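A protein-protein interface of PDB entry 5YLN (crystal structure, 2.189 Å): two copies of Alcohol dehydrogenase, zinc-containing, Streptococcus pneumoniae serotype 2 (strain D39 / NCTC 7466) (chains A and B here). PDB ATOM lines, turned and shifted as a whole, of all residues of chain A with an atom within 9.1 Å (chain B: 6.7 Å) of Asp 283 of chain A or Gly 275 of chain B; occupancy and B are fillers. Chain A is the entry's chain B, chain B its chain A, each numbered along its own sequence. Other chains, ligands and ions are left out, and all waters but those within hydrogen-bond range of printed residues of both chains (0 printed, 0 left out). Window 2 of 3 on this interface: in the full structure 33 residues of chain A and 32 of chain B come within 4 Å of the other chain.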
ATOM      1  N   GLN A 259      20.204  12.307 -22.901  1.00  0.00           N
ATOM      2  CA  GLN A 259      20.958  11.263 -23.588  1.00  0.00           C
ATOM      3  C   GLN A 259      20.250  10.769 -24.841  1.00  0.00           C
ATOM      4  O   GLN A 259      20.878  10.097 -25.661  1.00  0.00           O
ATOM      5  CB  GLN A 259      21.242  10.088 -22.642  1.00  0.00           C
ATOM      6  CG  GLN A 259      20.101   9.097 -22.476  1.00  0.00           C
ATOM      7  CD  GLN A 259      20.508   7.888 -21.635  1.00  0.00           C
ATOM      8  OE1 GLN A 259      21.676   7.486 -21.614  1.00  0.00           O
ATOM      9  NE2 GLN A 259      19.543   7.304 -20.945  1.00  0.00           N
ATOM     10  N   LYS A 260      18.972  11.098 -25.020  1.00  0.00           N
ATOM     11  CA  LYS A 260      18.264  10.694 -26.224  1.00  0.00           C
ATOM     12  C   LYS A 260      18.311  11.750 -27.315  1.00  0.00           C
ATOM     13  O   LYS A 260      18.102  11.425 -28.491  1.00  0.00           O
ATOM     14  CB  LYS A 260      16.807  10.351 -25.875  1.00  0.00           C
ATOM     15  CG  LYS A 260      16.647   8.898 -25.369  1.00  0.00           C
ATOM     16  CD  LYS A 260      15.342   8.692 -24.617  1.00  0.00           C
ATOM     17  CE  LYS A 260      15.090   7.195 -24.312  1.00  0.00           C
ATOM     18  NZ  LYS A 260      16.228   6.539 -23.595  1.00  0.00           N
ATOM     19  N   GLU A 279      19.841   5.435 -15.486  1.00  0.00           N
ATOM     20  CA  GLU A 279      20.178   4.466 -16.512  1.00  0.00           C
ATOM     21  C   GLU A 279      20.860   5.197 -17.659  1.00  0.00           C
ATOM     22  O   GLU A 279      20.301   6.139 -18.227  1.00  0.00           O
ATOM     23  CB  GLU A 279      18.944   3.716 -17.003  1.00  0.00           C
ATOM     24  CG  GLU A 279      19.225   2.887 -18.252  1.00  0.00           C
ATOM     25  CD  GLU A 279      18.101   1.911 -18.591  1.00  0.00           C
ATOM     26  OE1 GLU A 279      17.235   2.245 -19.435  1.00  0.00           O
ATOM     27  OE2 GLU A 279      18.093   0.804 -18.010  1.00  0.00           O
ATOM     28  N   PHE A 280      22.071   4.765 -17.977  1.00  0.00           N
ATOM     29  CA  PHE A 280      22.908   5.377 -18.995  1.00  0.00           C
ATOM     30  C   PHE A 280      22.990   4.392 -20.151  1.00  0.00           C
ATOM     31  O   PHE A 280      23.479   3.270 -19.976  1.00  0.00           O
ATOM     32  CB  PHE A 280      24.278   5.704 -18.394  1.00  0.00           C
ATOM     33  CG  PHE A 280      25.281   6.245 -19.365  1.00  0.00           C
ATOM     34  CD1 PHE A 280      24.940   7.233 -20.272  1.00  0.00           C
ATOM     35  CD2 PHE A 280      26.589   5.798 -19.325  1.00  0.00           C
ATOM     36  CE1 PHE A 280      25.881   7.733 -21.163  1.00  0.00           C
ATOM     37  CE2 PHE A 280      27.538   6.294 -20.204  1.00  0.00           C
ATOM     38  CZ  PHE A 280      27.186   7.267 -21.124  1.00  0.00           C
ATOM     39  N   ASP A 281      22.505   4.806 -21.327  1.00  0.00           N
ATOM     40  CA  ASP A 281      22.306   3.897 -22.459  1.00  0.00           C
ATOM     41  C   ASP A 281      23.592   3.660 -23.255  1.00  0.00           C
ATOM     42  O   ASP A 281      23.654   3.889 -24.463  1.00  0.00           O
ATOM     43  CB  ASP A 281      21.203   4.433 -23.363  1.00  0.00           C
ATOM     44  CG  ASP A 281      19.828   4.360 -22.717  1.00  0.00           C
ATOM     45  OD1 ASP A 281      19.500   3.310 -22.134  1.00  0.00           O
ATOM     46  OD2 ASP A 281      19.080   5.357 -22.796  1.00  0.00           O
ATOM     47  N   LEU A 282      24.620   3.144 -22.565  1.00  0.00           N
ATOM     48  CA  LEU A 282      25.892   2.854 -23.228  1.00  0.00           C
ATOM     49  C   LEU A 282      25.742   1.865 -24.374  1.00  0.00           C
ATOM     50  O   LEU A 282      26.593   1.849 -25.271  1.00  0.00           O
ATOM     51  CB  LEU A 282      26.920   2.302 -22.227  1.00  0.00           C
ATOM     52  CG  LEU A 282      28.029   3.175 -21.655  1.00  0.00           C
ATOM     53  CD1 LEU A 282      29.010   2.296 -20.894  1.00  0.00           C
ATOM     54  CD2 LEU A 282      28.739   3.982 -22.752  1.00  0.00           C
ATOM     55  N   ASP A 283      24.688   1.033 -24.363  1.00  0.00           N
ATOM     56  CA  ASP A 283      24.495   0.076 -25.448  1.00  0.00           C
ATOM     57  C   ASP A 283      24.205   0.791 -26.754  1.00  0.00           C
ATOM     58  O   ASP A 283      24.564   0.293 -27.826  1.00  0.00           O
ATOM     59  CB  ASP A 283      23.363  -0.900 -25.118  1.00  0.00           C
ATOM     60  CG  ASP A 283      22.029  -0.204 -24.898  1.00  0.00           C
ATOM     61  OD1 ASP A 283      22.001   0.806 -24.165  1.00  0.00           O
ATOM     62  OD2 ASP A 283      21.006  -0.669 -25.455  1.00  0.00           O
ATOM     63  N   LYS A 284      23.557   1.950 -26.678  1.00  0.00           N
ATOM     64  CA  LYS A 284      23.314   2.796 -27.835  1.00  0.00           C
ATOM     65  C   LYS A 284      24.413   3.834 -28.053  1.00  0.00           C
ATOM     66  O   LYS A 284      24.701   4.195 -29.202  1.00  0.00           O
ATOM     67  CB  LYS A 284      21.954   3.491 -27.678  1.00  0.00           C
ATOM     68  CG  LYS A 284      20.751   2.523 -27.552  1.00  0.00           C
ATOM     69  CD  LYS A 284      19.622   3.182 -26.742  1.00  0.00           C
ATOM     70  CE  LYS A 284      18.302   2.410 -26.787  1.00  0.00           C
ATOM     71  NZ  LYS A 284      17.292   3.059 -25.881  1.00  0.00           N
ATOM     72  N   LEU A 285      25.050   4.314 -26.986  1.00  0.00           N
ATOM     73  CA  LEU A 285      25.859   5.527 -27.042  1.00  0.00           C
ATOM     74  C   LEU A 285      27.361   5.271 -27.094  1.00  0.00           C
ATOM     75  O   LEU A 285      28.121   6.224 -27.295  1.00  0.00           O
ATOM     76  CB  LEU A 285      25.538   6.410 -25.826  1.00  0.00           C
ATOM     77  CG  LEU A 285      24.074   6.841 -25.774  1.00  0.00           C
ATOM     78  CD1 LEU A 285      23.677   7.311 -24.378  1.00  0.00           C
ATOM     79  CD2 LEU A 285      23.826   7.937 -26.809  1.00  0.00           C
ATOM     80  N   TRP A 286      27.810   4.023 -26.894  1.00  0.00           N
ATOM     81  CA  TRP A 286      29.228   3.725 -27.027  1.00  0.00           C
ATOM     82  C   TRP A 286      29.723   4.086 -28.416  1.00  0.00           C
ATOM     83  O   TRP A 286      30.879   4.480 -28.581  1.00  0.00           O
ATOM     84  CB  TRP A 286      29.502   2.246 -26.737  1.00  0.00           C
ATOM     85  CG  TRP A 286      29.107   1.346 -27.862  1.00  0.00           C
ATOM     86  CD1 TRP A 286      27.901   0.716 -28.029  1.00  0.00           C
ATOM     87  CD2 TRP A 286      29.910   0.984 -28.991  1.00  0.00           C
ATOM     88  NE1 TRP A 286      27.912  -0.019 -29.186  1.00  0.00           N
ATOM     89  CE2 TRP A 286      29.133   0.128 -29.796  1.00  0.00           C
ATOM     90  CE3 TRP A 286      31.216   1.300 -29.396  1.00  0.00           C
ATOM     91  CZ2 TRP A 286      29.616  -0.421 -30.981  1.00  0.00           C
ATOM     92  CZ3 TRP A 286      31.695   0.753 -30.564  1.00  0.00           C
ATOM     93  CH2 TRP A 286      30.899  -0.098 -31.347  1.00  0.00           C
ATOM     94  N   ILE A 287      28.849   3.989 -29.419  1.00  0.00           N
ATOM     95  CA  ILE A 287      29.230   4.224 -30.803  1.00  0.00           C
ATOM     96  C   ILE A 287      29.022   5.668 -31.241  1.00  0.00           C
ATOM     97  O   ILE A 287      29.547   6.067 -32.291  1.00  0.00           O
ATOM     98  CB  ILE A 287      28.438   3.240 -31.691  1.00  0.00           C
ATOM     99  CG1 ILE A 287      29.200   2.957 -32.992  1.00  0.00           C
ATOM    100  CG2 ILE A 287      27.018   3.768 -31.938  1.00  0.00           C
ATOM    101  CD1 ILE A 287      28.536   1.945 -33.873  1.00  0.00           C
ATOM    102  N   ARG A 288      28.322   6.482 -30.453  1.00  0.00           N
ATOM    103  CA  ARG A 288      27.919   7.820 -30.882  1.00  0.00           C
ATOM    104  C   ARG A 288      28.939   8.905 -30.555  1.00  0.00           C
ATOM    105  O   ARG A 288      28.714  10.071 -30.898  1.00  0.00           O
ATOM    106  CB  ARG A 288      26.571   8.173 -30.259  1.00  0.00           C
ATOM    107  CG  ARG A 288      25.826   9.315 -30.939  1.00  0.00           C
ATOM    108  CD  ARG A 288      24.383   9.239 -30.506  1.00  0.00           C
ATOM    109  NE  ARG A 288      23.552  10.348 -30.970  1.00  0.00           N
ATOM    110  CZ  ARG A 288      22.977  10.391 -32.170  1.00  0.00           C
ATOM    111  NH1 ARG A 288      23.190   9.407 -33.048  1.00  0.00           N
ATOM    112  NH2 ARG A 288      22.204  11.422 -32.504  1.00  0.00           N
ATOM    113  N   GLY B 250      33.694  -3.644 -21.621  1.00  0.00           N
ATOM    114  CA  GLY B 250      32.360  -3.426 -22.137  1.00  0.00           C
ATOM    115  C   GLY B 250      31.250  -4.190 -21.433  1.00  0.00           C
ATOM    116  O   GLY B 250      30.282  -4.584 -22.077  1.00  0.00           O
ATOM    117  N   ILE B 251      31.360  -4.411 -20.127  1.00  0.00           N
ATOM    118  CA  ILE B 251      30.248  -5.002 -19.388  1.00  0.00           C
ATOM    119  C   ILE B 251      29.914  -4.090 -18.217  1.00  0.00           C
ATOM    120  O   ILE B 251      30.717  -3.220 -17.827  1.00  0.00           O
ATOM    121  CB  ILE B 251      30.564  -6.442 -18.906  1.00  0.00           C
ATOM    122  CG1 ILE B 251      31.751  -6.448 -17.937  1.00  0.00           C
ATOM    123  CG2 ILE B 251      30.766  -7.395 -20.100  1.00  0.00           C
ATOM    124  CD1 ILE B 251      31.821  -7.698 -17.090  1.00  0.00           C
ATOM    125  N   PRO B 252      28.711  -4.242 -17.655  1.00  0.00           N
ATOM    126  CA  PRO B 252      28.318  -3.385 -16.524  1.00  0.00           C
ATOM    127  C   PRO B 252      29.279  -3.432 -15.353  1.00  0.00           C
ATOM    128  O   PRO B 252      29.452  -2.414 -14.674  1.00  0.00           O
ATOM    129  CB  PRO B 252      26.938  -3.936 -16.137  1.00  0.00           C
ATOM    130  CG  PRO B 252      26.401  -4.511 -17.417  1.00  0.00           C
ATOM    131  CD  PRO B 252      27.594  -5.068 -18.149  1.00  0.00           C
ATOM    132  N   VAL B 273      32.306  -2.043 -26.915  1.00  0.00           N
ATOM    133  CA  VAL B 273      30.879  -2.205 -27.134  1.00  0.00           C
ATOM    134  C   VAL B 273      30.213  -2.681 -25.850  1.00  0.00           C
ATOM    135  O   VAL B 273      30.721  -3.566 -25.152  1.00  0.00           O
ATOM    136  CB  VAL B 273      30.642  -3.218 -28.265  1.00  0.00           C
ATOM    137  CG1 VAL B 273      29.192  -3.199 -28.687  1.00  0.00           C
ATOM    138  CG2 VAL B 273      31.581  -2.919 -29.424  1.00  0.00           C
ATOM    139  N   HIS B 274      29.079  -2.077 -25.518  1.00  0.00           N
ATOM    140  CA  HIS B 274      28.245  -2.551 -24.426  1.00  0.00           C
ATOM    141  C   HIS B 274      26.957  -3.100 -25.016  1.00  0.00           C
ATOM    142  O   HIS B 274      26.395  -2.513 -25.944  1.00  0.00           O
ATOM    143  CB  HIS B 274      27.947  -1.438 -23.411  1.00  0.00           C
ATOM    144  CG  HIS B 274      29.118  -1.074 -22.549  1.00  0.00           C
ATOM    145  ND1 HIS B 274      29.192  -1.417 -21.215  1.00  0.00           N
ATOM    146  CD2 HIS B 274      30.265  -0.404 -22.833  1.00  0.00           C
ATOM    147  CE1 HIS B 274      30.329  -0.966 -20.712  1.00  0.00           C
ATOM    148  NE2 HIS B 274      30.998  -0.352 -21.673  1.00  0.00           N
ATOM    149  N   GLY B 275      26.516  -4.245 -24.507  1.00  0.00           N
ATOM    150  CA  GLY B 275      25.296  -4.851 -25.002  1.00  0.00           C
ATOM    151  C   GLY B 275      24.119  -4.561 -24.101  1.00  0.00           C
ATOM    152  O   GLY B 275      22.967  -4.840 -24.455  1.00  0.00           O
ATOM    153  N   LYS B 276      24.402  -4.004 -22.929  1.00  0.00           N
ATOM    154  CA  LYS B 276      23.379  -3.590 -21.983  1.00  0.00           C
ATOM    155  C   LYS B 276      23.635  -2.158 -21.550  1.00  0.00           C
ATOM    156  O   LYS B 276      24.781  -1.708 -21.546  1.00  0.00           O
ATOM    157  CB  LYS B 276      23.356  -4.479 -20.732  1.00  0.00           C
ATOM    158  CG  LYS B 276      22.733  -5.852 -20.931  1.00  0.00           C
ATOM    159  CD  LYS B 276      22.150  -6.376 -19.617  1.00  0.00           C
ATOM    160  CE  LYS B 276      23.186  -6.442 -18.501  1.00  0.00           C
ATOM    161  NZ  LYS B 276      24.368  -7.285 -18.865  1.00  0.00           N
ATOM    162  N   PRO B 277      22.593  -1.427 -21.163  1.00  0.00           N
ATOM    163  CA  PRO B 277      22.820  -0.136 -20.509  1.00  0.00           C
ATOM    164  C   PRO B 277      23.423  -0.366 -19.133  1.00  0.00           C
ATOM    165  O   PRO B 277      23.410  -1.476 -18.593  1.00  0.00           O
ATOM    166  CB  PRO B 277      21.420   0.486 -20.418  1.00  0.00           C
ATOM    167  CG  PRO B 277      20.496  -0.689 -20.394  1.00  0.00           C
ATOM    168  CD  PRO B 277      21.161  -1.765 -21.247  1.00  0.00           C
ATOM    169  N   VAL B 278      23.987   0.698 -18.571  1.00  0.00           N
ATOM    170  CA  VAL B 278      24.676   0.575 -17.298  1.00  0.00           C
ATOM    171  C   VAL B 278      24.064   1.558 -16.311  1.00  0.00           C
ATOM    172  O   VAL B 278      23.402   2.527 -16.690  1.00  0.00           O
ATOM    173  CB  VAL B 278      26.191   0.793 -17.444  1.00  0.00           C
ATOM    174  CG1 VAL B 278      26.811  -0.316 -18.328  1.00  0.00           C
ATOM    175  CG2 VAL B 278      26.470   2.192 -18.015  1.00  0.00           C
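Asp 283 of chain A touches four residues of chain B. Gly 275 of chain B touches just one residue of chain A: Asp 283. Of the printed residues of chain A, Val 278 of chain B touches Glu 279, Phe 280 and Leu 282. Printed residues of chain A within 4 Å of His 274 of chain B: Leu 282, Asp 283 and Trp 286. Gly 250 of chain B touches none of the printed residues of chain A. The nearest residue of chain A that does not touch Gly 275 of chain B is Leu 282 of chain A (6.1 Å). The nearest printed residue of chain A that does not touch Pro 277 of chain B is Leu 282 of chain A (4.3 Å).
Of the 9 printed residues of chain B, 6 touch a printed residue of chain A. Along chain B the printed residues that touch a printed residue of chain A span positions 273 to 278. Among the printed residues, 13 pairs touch across the chains. Among the printed residues, no Asp or Glu carboxylate lies within 4 Å of a Lys or Arg side-chain nitrogen of the other chain.
No position is printed for both chains.
NE2 of Gln 259 of chain A is in hydrogen-bond range of O of Glu 279 of chain A (3.1 Å). The side-chain carboxylate (OD2) of Asp 281 of chain A lies within salt-bridge range of the side-chain amino group (NZ) of Lys 260 of chain A (3.2 Å). NE2 of Gln 259 of chain A sits at hydrogen-bond distance from OD2 of Asp 281 of chain A. O of Gly 250 of chain B lies within hydrogen-bond range of ND1 of His 274 of chain B, at 3.5 Å.
Among the printed residues, pairs that only touch across the chains: Asp 283 of chain A with His 274 of chain B (3.2 Å), Leu 282 of chain A with His 274 of chain B (3.4 Å), Trp 286 of chain A with Val 273 of chain B (3.5 Å), Phe 280 of chain A with Pro 277 of chain B (3.5 Å), Glu 279 of chain A with Pro 277 of chain B (3.7 Å), Glu 279 of chain A with Val 278 of chain B (3.8 Å), Asp 283 of chain A with Pro 277 of chain B (3.8 Å), Asp 283 of chain A with Lys 276 of chain B (3.8 Å), Asp 281 of chain A with Pro 277 of chain B (3.8 Å), Leu 282 of chain A with Val 278 of chain B (3.8 Å), Asp 283 of chain A with Gly 275 of chain B (3.9 Å) and Trp 286 of chain A with His 274 of chain B (3.9 Å).
O of Val 278 of chain B lies within hydrogen-bond range of N of Phe 280 of chain A (2.9 Å).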
